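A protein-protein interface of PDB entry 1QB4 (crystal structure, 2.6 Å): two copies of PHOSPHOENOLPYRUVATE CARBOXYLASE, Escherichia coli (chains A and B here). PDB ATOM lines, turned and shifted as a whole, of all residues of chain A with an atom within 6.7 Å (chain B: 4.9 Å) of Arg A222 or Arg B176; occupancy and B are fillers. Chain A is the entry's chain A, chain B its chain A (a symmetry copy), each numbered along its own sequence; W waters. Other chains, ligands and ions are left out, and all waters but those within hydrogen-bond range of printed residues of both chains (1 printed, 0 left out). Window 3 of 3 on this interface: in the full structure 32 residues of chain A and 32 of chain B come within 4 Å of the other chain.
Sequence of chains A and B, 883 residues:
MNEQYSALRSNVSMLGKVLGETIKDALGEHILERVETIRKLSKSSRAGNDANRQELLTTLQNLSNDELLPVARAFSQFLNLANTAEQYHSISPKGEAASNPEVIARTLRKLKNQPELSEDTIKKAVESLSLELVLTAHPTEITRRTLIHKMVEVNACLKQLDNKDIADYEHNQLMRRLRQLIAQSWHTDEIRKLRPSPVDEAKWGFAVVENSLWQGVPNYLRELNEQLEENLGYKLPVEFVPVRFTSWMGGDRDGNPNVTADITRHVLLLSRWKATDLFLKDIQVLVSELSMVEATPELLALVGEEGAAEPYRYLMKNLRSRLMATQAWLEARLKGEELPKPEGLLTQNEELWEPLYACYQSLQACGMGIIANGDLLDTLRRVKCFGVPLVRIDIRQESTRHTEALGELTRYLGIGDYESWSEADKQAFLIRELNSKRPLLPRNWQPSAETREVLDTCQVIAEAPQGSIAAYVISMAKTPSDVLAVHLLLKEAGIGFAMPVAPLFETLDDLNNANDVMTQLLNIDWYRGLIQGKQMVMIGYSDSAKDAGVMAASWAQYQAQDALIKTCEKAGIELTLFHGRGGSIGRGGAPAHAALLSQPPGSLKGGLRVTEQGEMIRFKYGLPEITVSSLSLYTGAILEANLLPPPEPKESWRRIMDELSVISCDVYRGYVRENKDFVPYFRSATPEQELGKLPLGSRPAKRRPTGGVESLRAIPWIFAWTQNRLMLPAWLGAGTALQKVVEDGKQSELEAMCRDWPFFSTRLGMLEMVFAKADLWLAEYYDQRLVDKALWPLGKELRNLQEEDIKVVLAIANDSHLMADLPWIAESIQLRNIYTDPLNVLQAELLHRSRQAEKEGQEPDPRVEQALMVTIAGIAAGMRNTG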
ATOM      1  N   VAL A 217      -0.299  25.388  17.108  1.00  0.00           N
ATOM      2  CA  VAL A 217      -0.268  23.935  17.247  1.00  0.00           C
ATOM      3  C   VAL A 217       1.063  23.308  17.128  1.00  0.00           C
ATOM      4  O   VAL A 217       1.484  22.537  18.032  1.00  0.00           O
ATOM      5  CB  VAL A 217      -1.415  23.256  16.497  1.00  0.00           C
ATOM      6  CG1 VAL A 217      -1.325  21.766  16.727  1.00  0.00           C
ATOM      7  CG2 VAL A 217      -2.714  23.870  17.079  1.00  0.00           C
ATOM      8  N   PRO A 218       1.803  23.577  16.081  1.00  0.00           N
ATOM      9  CA  PRO A 218       3.134  22.993  15.888  1.00  0.00           C
ATOM     10  C   PRO A 218       4.073  23.342  17.022  1.00  0.00           C
ATOM     11  O   PRO A 218       4.854  22.463  17.394  1.00  0.00           O
ATOM     12  CB  PRO A 218       3.579  23.492  14.535  1.00  0.00           C
ATOM     13  CG  PRO A 218       2.308  23.843  13.837  1.00  0.00           C
ATOM     14  CD  PRO A 218       1.385  24.402  14.924  1.00  0.00           C
ATOM     15  N   ASN A 219       4.030  24.507  17.625  1.00  0.00           N
ATOM     16  CA  ASN A 219       4.883  24.869  18.747  1.00  0.00           C
ATOM     17  C   ASN A 219       4.528  24.026  19.949  1.00  0.00           C
ATOM     18  O   ASN A 219       5.378  23.452  20.609  1.00  0.00           O
ATOM     19  CB  ASN A 219       4.758  26.338  19.128  1.00  0.00           C
ATOM     20  CG  ASN A 219       5.299  27.364  18.148  1.00  0.00           C
ATOM     21  OD1 ASN A 219       5.979  27.106  17.186  1.00  0.00           O
ATOM     22  ND2 ASN A 219       4.984  28.618  18.341  1.00  0.00           N
ATOM     23  N   TYR A 220       3.213  23.867  20.161  1.00  0.00           N
ATOM     24  CA  TYR A 220       2.712  23.025  21.269  1.00  0.00           C
ATOM     25  C   TYR A 220       3.331  21.643  21.043  1.00  0.00           C
ATOM     26  O   TYR A 220       3.932  21.126  21.993  1.00  0.00           O
ATOM     27  CB  TYR A 220       1.216  22.982  21.385  1.00  0.00           C
ATOM     28  CG  TYR A 220       0.693  21.610  21.802  1.00  0.00           C
ATOM     29  CD1 TYR A 220      -0.045  20.852  20.901  1.00  0.00           C
ATOM     30  CD2 TYR A 220       0.941  21.075  23.044  1.00  0.00           C
ATOM     31  CE1 TYR A 220      -0.522  19.612  21.244  1.00  0.00           C
ATOM     32  CE2 TYR A 220       0.456  19.855  23.428  1.00  0.00           C
ATOM     33  CZ  TYR A 220      -0.285  19.129  22.521  1.00  0.00           C
ATOM     34  OH  TYR A 220      -0.777  17.905  22.870  1.00  0.00           O
ATOM     35  N   LEU A 221       3.256  21.122  19.828  1.00  0.00           N
ATOM     36  CA  LEU A 221       3.827  19.809  19.554  1.00  0.00           C
ATOM     37  C   LEU A 221       5.319  19.718  19.690  1.00  0.00           C
ATOM     38  O   LEU A 221       5.863  18.618  19.962  1.00  0.00           O
ATOM     39  CB  LEU A 221       3.477  19.334  18.130  1.00  0.00           C
ATOM     40  CG  LEU A 221       2.000  18.907  17.996  1.00  0.00           C
ATOM     41  CD1 LEU A 221       1.385  19.660  16.835  1.00  0.00           C
ATOM     42  CD2 LEU A 221       1.837  17.414  17.802  1.00  0.00           C
ATOM     43  N   ARG A 222       6.056  20.804  19.483  1.00  0.00           N
ATOM     44  CA  ARG A 222       7.539  20.699  19.629  1.00  0.00           C
ATOM     45  C   ARG A 222       7.897  20.660  21.093  1.00  0.00           C
ATOM     46  O   ARG A 222       8.681  19.861  21.572  1.00  0.00           O
ATOM     47  CB  ARG A 222       8.076  21.902  18.933  1.00  0.00           C
ATOM     48  CG  ARG A 222       9.298  21.800  18.045  1.00  0.00           C
ATOM     49  CD  ARG A 222       9.392  22.931  17.103  1.00  0.00           C
ATOM     50  NE  ARG A 222       9.248  22.801  15.673  1.00  0.00           N
ATOM     51  CZ  ARG A 222      10.029  22.012  14.916  1.00  0.00           C
ATOM     52  NH1 ARG A 222      10.977  21.286  15.518  1.00  0.00           N
ATOM     53  NH2 ARG A 222       9.843  21.952  13.627  1.00  0.00           N
ATOM     54  N   GLU A 223       7.341  21.553  21.876  1.00  0.00           N
ATOM     55  CA  GLU A 223       7.565  21.635  23.303  1.00  0.00           C
ATOM     56  C   GLU A 223       7.183  20.329  23.951  1.00  0.00           C
ATOM     57  O   GLU A 223       7.996  19.747  24.687  1.00  0.00           O
ATOM     58  CB  GLU A 223       6.799  22.856  23.821  1.00  0.00           C
ATOM     59  CG  GLU A 223       7.416  24.213  23.714  1.00  0.00           C
ATOM     60  CD  GLU A 223       8.886  24.271  23.339  1.00  0.00           C
ATOM     61  OE1 GLU A 223       9.792  23.877  24.099  1.00  0.00           O
ATOM     62  OE2 GLU A 223       9.164  24.734  22.192  1.00  0.00           O
ATOM     63  N   LEU A 224       5.981  19.798  23.679  1.00  0.00           N
ATOM     64  CA  LEU A 224       5.507  18.535  24.232  1.00  0.00           C
ATOM     65  C   LEU A 224       6.514  17.441  23.876  1.00  0.00           C
ATOM     66  O   LEU A 224       6.819  16.579  24.687  1.00  0.00           O
ATOM     67  CB  LEU A 224       4.177  18.092  23.650  1.00  0.00           C
ATOM     68  CG  LEU A 224       3.707  16.659  23.914  1.00  0.00           C
ATOM     69  CD1 LEU A 224       3.282  16.538  25.363  1.00  0.00           C
ATOM     70  CD2 LEU A 224       2.532  16.312  23.001  1.00  0.00           C
ATOM     71  N   ASN A 225       7.028  17.488  22.651  1.00  0.00           N
ATOM     72  CA  ASN A 225       7.989  16.478  22.281  1.00  0.00           C
ATOM     73  C   ASN A 225       9.326  16.628  22.957  1.00  0.00           C
ATOM     74  O   ASN A 225       9.973  15.669  23.387  1.00  0.00           O
ATOM     75  CB  ASN A 225       8.141  16.413  20.773  1.00  0.00           C
ATOM     76  CG  ASN A 225       7.659  15.086  20.246  1.00  0.00           C
ATOM     77  OD1 ASN A 225       6.512  14.680  20.334  1.00  0.00           O
ATOM     78  ND2 ASN A 225       8.614  14.338  19.700  1.00  0.00           N
ATOM     79  N   GLU A 226       9.795  17.855  23.087  1.00  0.00           N
ATOM     80  CA  GLU A 226      11.081  18.066  23.747  1.00  0.00           C
ATOM     81  C   GLU A 226      10.909  17.575  25.179  1.00  0.00           C
ATOM     82  O   GLU A 226      11.804  16.956  25.712  1.00  0.00           O
ATOM     83  CB  GLU A 226      11.428  19.533  23.716  1.00  0.00           C
ATOM     84  CG  GLU A 226      12.740  19.960  23.159  1.00  0.00           C
ATOM     85  CD  GLU A 226      12.624  20.645  21.811  1.00  0.00           C
ATOM     86  OE1 GLU A 226      12.736  19.950  20.778  1.00  0.00           O
ATOM     87  OE2 GLU A 226      12.428  21.880  21.762  1.00  0.00           O
ATOM     88  N   GLN A 227       9.777  17.852  25.812  1.00  0.00           N
ATOM     89  CA  GLN A 227       9.570  17.410  27.199  1.00  0.00           C
ATOM     90  C   GLN A 227       9.475  15.921  27.375  1.00  0.00           C
ATOM     91  O   GLN A 227      10.017  15.342  28.341  1.00  0.00           O
ATOM     92  CB  GLN A 227       8.332  18.179  27.672  1.00  0.00           C
ATOM     93  CG  GLN A 227       8.639  19.670  27.650  1.00  0.00           C
ATOM     94  CD  GLN A 227       9.510  20.038  28.835  1.00  0.00           C
ATOM     95  OE1 GLN A 227       8.949  19.964  29.936  1.00  0.00           O
ATOM     96  NE2 GLN A 227      10.743  20.426  28.689  1.00  0.00           N
ATOM     97  N   ILE A 370      18.012  17.888  10.756  1.00  0.00           N
ATOM     98  CA  ILE A 370      17.707  19.239  11.178  1.00  0.00           C
ATOM     99  C   ILE A 370      16.807  19.994  10.219  1.00  0.00           C
ATOM    100  O   ILE A 370      16.024  20.826  10.706  1.00  0.00           O
ATOM    101  CB  ILE A 370      18.968  20.114  11.434  1.00  0.00           C
ATOM    102  CG1 ILE A 370      20.056  19.297  12.110  1.00  0.00           C
ATOM    103  CG2 ILE A 370      18.646  21.248  12.385  1.00  0.00           C
ATOM    104  CD1 ILE A 370      21.371  20.017  12.358  1.00  0.00           C
ATOM    105  N   ALA A 372      14.665  18.524   8.033  1.00  0.00           N
ATOM    106  CA  ALA A 372      13.429  17.756   8.017  1.00  0.00           C
ATOM    107  C   ALA A 372      12.616  18.186   9.217  1.00  0.00           C
ATOM    108  O   ALA A 372      11.495  18.607   8.968  1.00  0.00           O
ATOM    109  CB  ALA A 372      13.712  16.271   8.007  1.00  0.00           C
ATOM    110  N   ASN A 373      13.200  18.224  10.412  1.00  0.00           N
ATOM    111  CA  ASN A 373      12.491  18.584  11.601  1.00  0.00           C
ATOM    112  C   ASN A 373      12.153  20.035  11.817  1.00  0.00           C
ATOM    113  O   ASN A 373      11.797  20.394  12.965  1.00  0.00           O
ATOM    114  CB  ASN A 373      13.256  18.137  12.891  1.00  0.00           C
ATOM    115  CG  ASN A 373      12.977  16.651  13.113  1.00  0.00           C
ATOM    116  OD1 ASN A 373      11.832  16.284  13.415  1.00  0.00           O
ATOM    117  ND2 ASN A 373      14.006  15.848  12.948  1.00  0.00           N
ATOM    118  N   GLY A 374      12.244  20.840  10.794  1.00  0.00           N
ATOM    119  CA  GLY A 374      11.996  22.251  10.829  1.00  0.00           C
ATOM    120  C   GLY A 374      10.681  22.558  10.163  1.00  0.00           C
ATOM    121  O   GLY A 374       9.708  21.965  10.607  1.00  0.00           O
ATOM    122  N   ASP A 375      10.599  23.386   9.151  1.00  0.00           N
ATOM    123  CA  ASP A 375       9.336  23.706   8.547  1.00  0.00           C
ATOM    124  C   ASP A 375       8.532  22.583   7.921  1.00  0.00           C
ATOM    125  O   ASP A 375       7.340  22.801   7.685  1.00  0.00           O
ATOM    126  CB  ASP A 375       9.538  24.789   7.467  1.00  0.00           C
ATOM    127  CG  ASP A 375      10.056  26.069   8.092  1.00  0.00           C
ATOM    128  OD1 ASP A 375       9.238  26.914   8.488  1.00  0.00           O
ATOM    129  OD2 ASP A 375      11.293  26.216   8.179  1.00  0.00           O
ATOM    130  N   LEU A 376       9.125  21.477   7.550  1.00  0.00           N
ATOM    131  CA  LEU A 376       8.459  20.323   6.975  1.00  0.00           C
ATOM    132  C   LEU A 376       7.584  19.677   8.086  1.00  0.00           C
ATOM    133  O   LEU A 376       6.387  19.522   7.896  1.00  0.00           O
ATOM    134  CB  LEU A 376       9.492  19.356   6.460  1.00  0.00           C
ATOM    135  CG  LEU A 376       9.052  18.339   5.412  1.00  0.00           C
ATOM    136  CD1 LEU A 376       8.182  18.929   4.305  1.00  0.00           C
ATOM    137  CD2 LEU A 376      10.274  17.678   4.851  1.00  0.00           C
ATOM    138  N   LEU A 377       8.191  19.455   9.239  1.00  0.00           N
ATOM    139  CA  LEU A 377       7.587  18.932  10.435  1.00  0.00           C
ATOM    140  C   LEU A 377       6.358  19.787  10.762  1.00  0.00           C
ATOM    141  O   LEU A 377       5.237  19.323  10.989  1.00  0.00           O
ATOM    142  CB  LEU A 377       8.567  18.938  11.595  1.00  0.00           C
ATOM    143  CG  LEU A 377       8.189  18.111  12.793  1.00  0.00           C
ATOM    144  CD1 LEU A 377       7.528  16.771  12.406  1.00  0.00           C
ATOM    145  CD2 LEU A 377       9.376  17.849  13.680  1.00  0.00           C
ATOM    146  N   ASP A 378       6.539  21.108  10.698  1.00  0.00           N
ATOM    147  CA  ASP A 378       5.422  21.996  10.984  1.00  0.00           C
ATOM    148  C   ASP A 378       4.304  21.811  10.005  1.00  0.00           C
ATOM    149  O   ASP A 378       3.115  21.904  10.348  1.00  0.00           O
ATOM    150  CB  ASP A 378       5.930  23.436  11.003  1.00  0.00           C
ATOM    151  CG  ASP A 378       6.575  23.845  12.284  1.00  0.00           C
ATOM    152  OD1 ASP A 378       7.069  23.028  13.112  1.00  0.00           O
ATOM    153  OD2 ASP A 378       6.603  25.069  12.523  1.00  0.00           O
ATOM    154  N   ARG A 381       2.488  18.289  10.614  1.00  0.00           N
ATOM    155  CA  ARG A 381       1.607  18.316  11.768  1.00  0.00           C
ATOM    156  C   ARG A 381       0.375  19.122  11.460  1.00  0.00           C
ATOM    157  O   ARG A 381      -0.691  18.764  11.969  1.00  0.00           O
ATOM    158  CB  ARG A 381       2.354  18.842  13.020  1.00  0.00           C
ATOM    159  CG  ARG A 381       3.689  18.085  13.165  1.00  0.00           C
ATOM    160  CD  ARG A 381       4.378  18.499  14.445  1.00  0.00           C
ATOM    161  NE  ARG A 381       5.196  17.394  14.902  1.00  0.00           N
ATOM    162  CZ  ARG A 381       6.148  17.508  15.826  1.00  0.00           C
ATOM    163  NH1 ARG A 381       6.381  18.676  16.372  1.00  0.00           N
ATOM    164  NH2 ARG A 381       6.849  16.471  16.216  1.00  0.00           N
ATOM    165  N   ASN B 172      16.136  28.863  24.420  1.00  0.00           N
ATOM    166  CA  ASN B 172      16.174  27.542  23.811  1.00  0.00           C
ATOM    167  C   ASN B 172      15.492  27.571  22.450  1.00  0.00           C
ATOM    168  O   ASN B 172      15.980  26.972  21.480  1.00  0.00           O
ATOM    169  CB  ASN B 172      15.424  26.670  24.844  1.00  0.00           C
ATOM    170  CG  ASN B 172      15.569  25.203  24.498  1.00  0.00           C
ATOM    171  OD1 ASN B 172      14.849  24.683  23.626  1.00  0.00           O
ATOM    172  ND2 ASN B 172      16.543  24.626  25.198  1.00  0.00           N
ATOM    173  N   GLN B 173      14.354  28.256  22.362  1.00  0.00           N
ATOM    174  CA  GLN B 173      13.561  28.368  21.139  1.00  0.00           C
ATOM    175  C   GLN B 173      14.340  29.082  20.025  1.00  0.00           C
ATOM    176  O   GLN B 173      14.432  28.618  18.882  1.00  0.00           O
ATOM    177  CB  GLN B 173      12.230  29.038  21.416  1.00  0.00           C
ATOM    178  CG  GLN B 173      11.212  28.229  22.146  1.00  0.00           C
ATOM    179  CD  GLN B 173      10.061  28.916  22.821  1.00  0.00           C
ATOM    180  OE1 GLN B 173       9.671  30.052  22.596  1.00  0.00           O
ATOM    181  NE2 GLN B 173       9.372  28.254  23.765  1.00  0.00           N
ATOM    182  N   LEU B 174      14.931  30.211  20.446  1.00  0.00           N
ATOM    183  CA  LEU B 174      15.774  31.044  19.580  1.00  0.00           C
ATOM    184  C   LEU B 174      16.954  30.236  19.074  1.00  0.00           C
ATOM    185  O   LEU B 174      17.225  30.088  17.887  1.00  0.00           O
ATOM    186  CB  LEU B 174      16.247  32.245  20.387  1.00  0.00           C
ATOM    187  CG  LEU B 174      15.193  33.344  20.575  1.00  0.00           C
ATOM    188  CD1 LEU B 174      15.807  34.510  21.284  1.00  0.00           C
ATOM    189  CD2 LEU B 174      14.578  33.718  19.240  1.00  0.00           C
ATOM    190  N   MET B 175      17.683  29.591  19.979  1.00  0.00           N
ATOM    191  CA  MET B 175      18.778  28.761  19.516  1.00  0.00           C
ATOM    192  C   MET B 175      18.296  27.674  18.570  1.00  0.00           C
ATOM    193  O   MET B 175      18.979  27.249  17.637  1.00  0.00           O
ATOM    194  CB  MET B 175      19.547  28.150  20.714  1.00  0.00           C
ATOM    195  CG  MET B 175      20.386  29.209  21.432  1.00  0.00           C
ATOM    196  SD  MET B 175      21.692  29.903  20.362  1.00  0.00           S
ATOM    197  CE  MET B 175      22.783  28.477  20.374  1.00  0.00           C
ATOM    198  N   ARG B 176      17.104  27.103  18.737  1.00  0.00           N
ATOM    199  CA  ARG B 176      16.638  26.023  17.841  1.00  0.00           C
ATOM    200  C   ARG B 176      16.430  26.525  16.427  1.00  0.00           C
ATOM    201  O   ARG B 176      16.700  25.836  15.475  1.00  0.00           O
ATOM    202  CB  ARG B 176      15.409  25.375  18.424  1.00  0.00           C
ATOM    203  CG  ARG B 176      14.700  24.277  17.611  1.00  0.00           C
ATOM    204  CD  ARG B 176      13.568  23.745  18.539  1.00  0.00           C
ATOM    205  NE  ARG B 176      12.454  24.685  18.623  1.00  0.00           N
ATOM    206  CZ  ARG B 176      11.768  25.038  19.694  1.00  0.00           C
ATOM    207  NH1 ARG B 176      12.011  24.574  20.908  1.00  0.00           N
ATOM    208  NH2 ARG B 176      10.758  25.918  19.589  1.00  0.00           N
ATOM    209  N   ARG B 177      15.931  27.739  16.276  1.00  0.00           N
ATOM    210  CA  ARG B 177      15.750  28.305  14.937  1.00  0.00           C
ATOM    211  C   ARG B 177      17.154  28.629  14.401  1.00  0.00           C
ATOM    212  O   ARG B 177      17.490  28.269  13.272  1.00  0.00           O
ATOM    213  CB  ARG B 177      14.877  29.530  14.937  1.00  0.00           C
ATOM    214  CG  ARG B 177      14.490  30.121  13.606  1.00  0.00           C
ATOM    215  CD  ARG B 177      13.994  29.135  12.563  1.00  0.00           C
ATOM    216  NE  ARG B 177      13.235  29.797  11.517  1.00  0.00           N
ATOM    217  CZ  ARG B 177      13.060  29.534  10.239  1.00  0.00           C
ATOM    218  NH1 ARG B 177      13.595  28.516   9.578  1.00  0.00           N
ATOM    219  NH2 ARG B 177      12.286  30.347   9.510  1.00  0.00           N
ATOM    220  N   LEU B 178      17.993  29.258  15.229  1.00  0.00           N
ATOM    221  CA  LEU B 178      19.363  29.553  14.786  1.00  0.00           C
ATOM    222  C   LEU B 178      20.029  28.314  14.195  1.00  0.00           C
ATOM    223  O   LEU B 178      20.649  28.440  13.120  1.00  0.00           O
ATOM    224  CB  LEU B 178      20.232  30.094  15.875  1.00  0.00           C
ATOM    225  CG  LEU B 178      21.044  31.362  15.661  1.00  0.00           C
ATOM    226  CD1 LEU B 178      22.407  31.172  16.294  1.00  0.00           C
ATOM    227  CD2 LEU B 178      21.137  31.771  14.207  1.00  0.00           C
ATOM    228  N   ARG B 179      19.909  27.149  14.826  1.00  0.00           N
ATOM    229  CA  ARG B 179      20.542  25.925  14.299  1.00  0.00           C
ATOM    230  C   ARG B 179      19.896  25.521  12.966  1.00  0.00           C
ATOM    231  O   ARG B 179      20.520  25.062  11.993  1.00  0.00           O
ATOM    232  CB  ARG B 179      20.503  24.910  15.359  1.00  0.00           C
ATOM    233  CG  ARG B 179      21.108  23.547  15.223  1.00  0.00           C
ATOM    234  CD  ARG B 179      21.529  23.107  16.646  1.00  0.00           C
ATOM    235  NE  ARG B 179      22.814  22.356  16.546  1.00  0.00           N
ATOM    236  CZ  ARG B 179      22.754  21.042  16.271  1.00  0.00           C
ATOM    237  NH1 ARG B 179      21.522  20.521  16.113  1.00  0.00           N
ATOM    238  NH2 ARG B 179      23.815  20.264  16.149  1.00  0.00           N
ATOM    239  N   GLN B 180      18.588  25.742  12.856  1.00  0.00           N
ATOM    240  CA  GLN B 180      17.862  25.449  11.637  1.00  0.00           C
ATOM    241  C   GLN B 180      18.433  26.302  10.503  1.00  0.00           C
ATOM    242  O   GLN B 180      18.886  25.866   9.435  1.00  0.00           O
ATOM    243  CB  GLN B 180      16.364  25.730  11.867  1.00  0.00           C
ATOM    244  CG  GLN B 180      15.495  24.507  11.528  1.00  0.00           C
ATOM    245  CD  GLN B 180      14.287  24.384  12.443  1.00  0.00           C
ATOM    246  OE1 GLN B 180      13.526  25.359  12.626  1.00  0.00           O
ATOM    247  NE2 GLN B 180      14.091  23.189  13.030  1.00  0.00           N
HETATM  248  O   HOH W   1      12.265  28.959   6.879  1.00  0.00           O
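Among the printed residues, pairs that only touch across the chains: Arg A222 with Arg B176, Glu A223 with Gln B173, Ile A370 with Arg B179, Ile A370 with Gln B180, Asn A373 with Gln B180 and Gly A374 with Gln B180.
Printed residues of chain A that touch a printed residue of chain B: Arg A222, Glu A223, Glu A226, Ile A370, Asn A373, Gly A374 and Asp A375.
Hydrophobic or aromatic side chains of chain A within 4 Å of the printed part of chain B: Ile A370.
Among the printed residues, Asp or Glu carboxylates within 4 Å of a Lys or Arg side-chain nitrogen of the other chain: Glu A223 with Arg B176 (3.1 Å), Glu A226 with Arg B176 (2.9 Å) and Asp A375 with Arg B177 (3.5 Å).
No position is printed for both chains.
Of the 9 pairs that touch across the chains among the printed residues, none has its exchanged pair printed and touching as well.
NH2 of Arg A222 is in hydrogen-bond range of O of Asn A373, 2.6 Å away.
NH2 of Arg A222 sits at hydrogen-bond distance from O of Gly A374.
OD1 of Asp A378 lies within salt-bridge range of NH2 of Arg A222, 3.0 Å away.
Water W1 lies within hydrogen-bond range of the guanidinium group of Arg B177 (3.0 Å) and the side-chain carboxylate of Asp A375 (3.2 Å).
Of the printed residues of chain B, Ile A370 touches Arg B179 (3.8 Å) and Gln B180 (3.8 Å).
Of the printed residues of chain B, Asp A375 touches Arg B177 (3.5 Å).
Of chain A, only Arg A222, Glu A223 and Glu A226 come within 4 Å of Arg B176.
The nearest residue of chain B that does not touch Arg A222 is Gln B180 (4.4 Å).
The nearest residue of chain A that does not touch Arg B176 is Asn A219 (5.5 Å).
The guanidinium group (NH1) of Arg B176 lies within salt-bridge range of the side-chain carboxylate (OE2) of Glu A223 (3.1 Å).
The guanidinium group (NH1) of Arg B176 is in salt-bridge range of the side-chain carboxylate (OE2) of Glu A226.
NH1 of Arg B177 is in salt-bridge range of OD2 of Asp A375 (3.5 Å).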
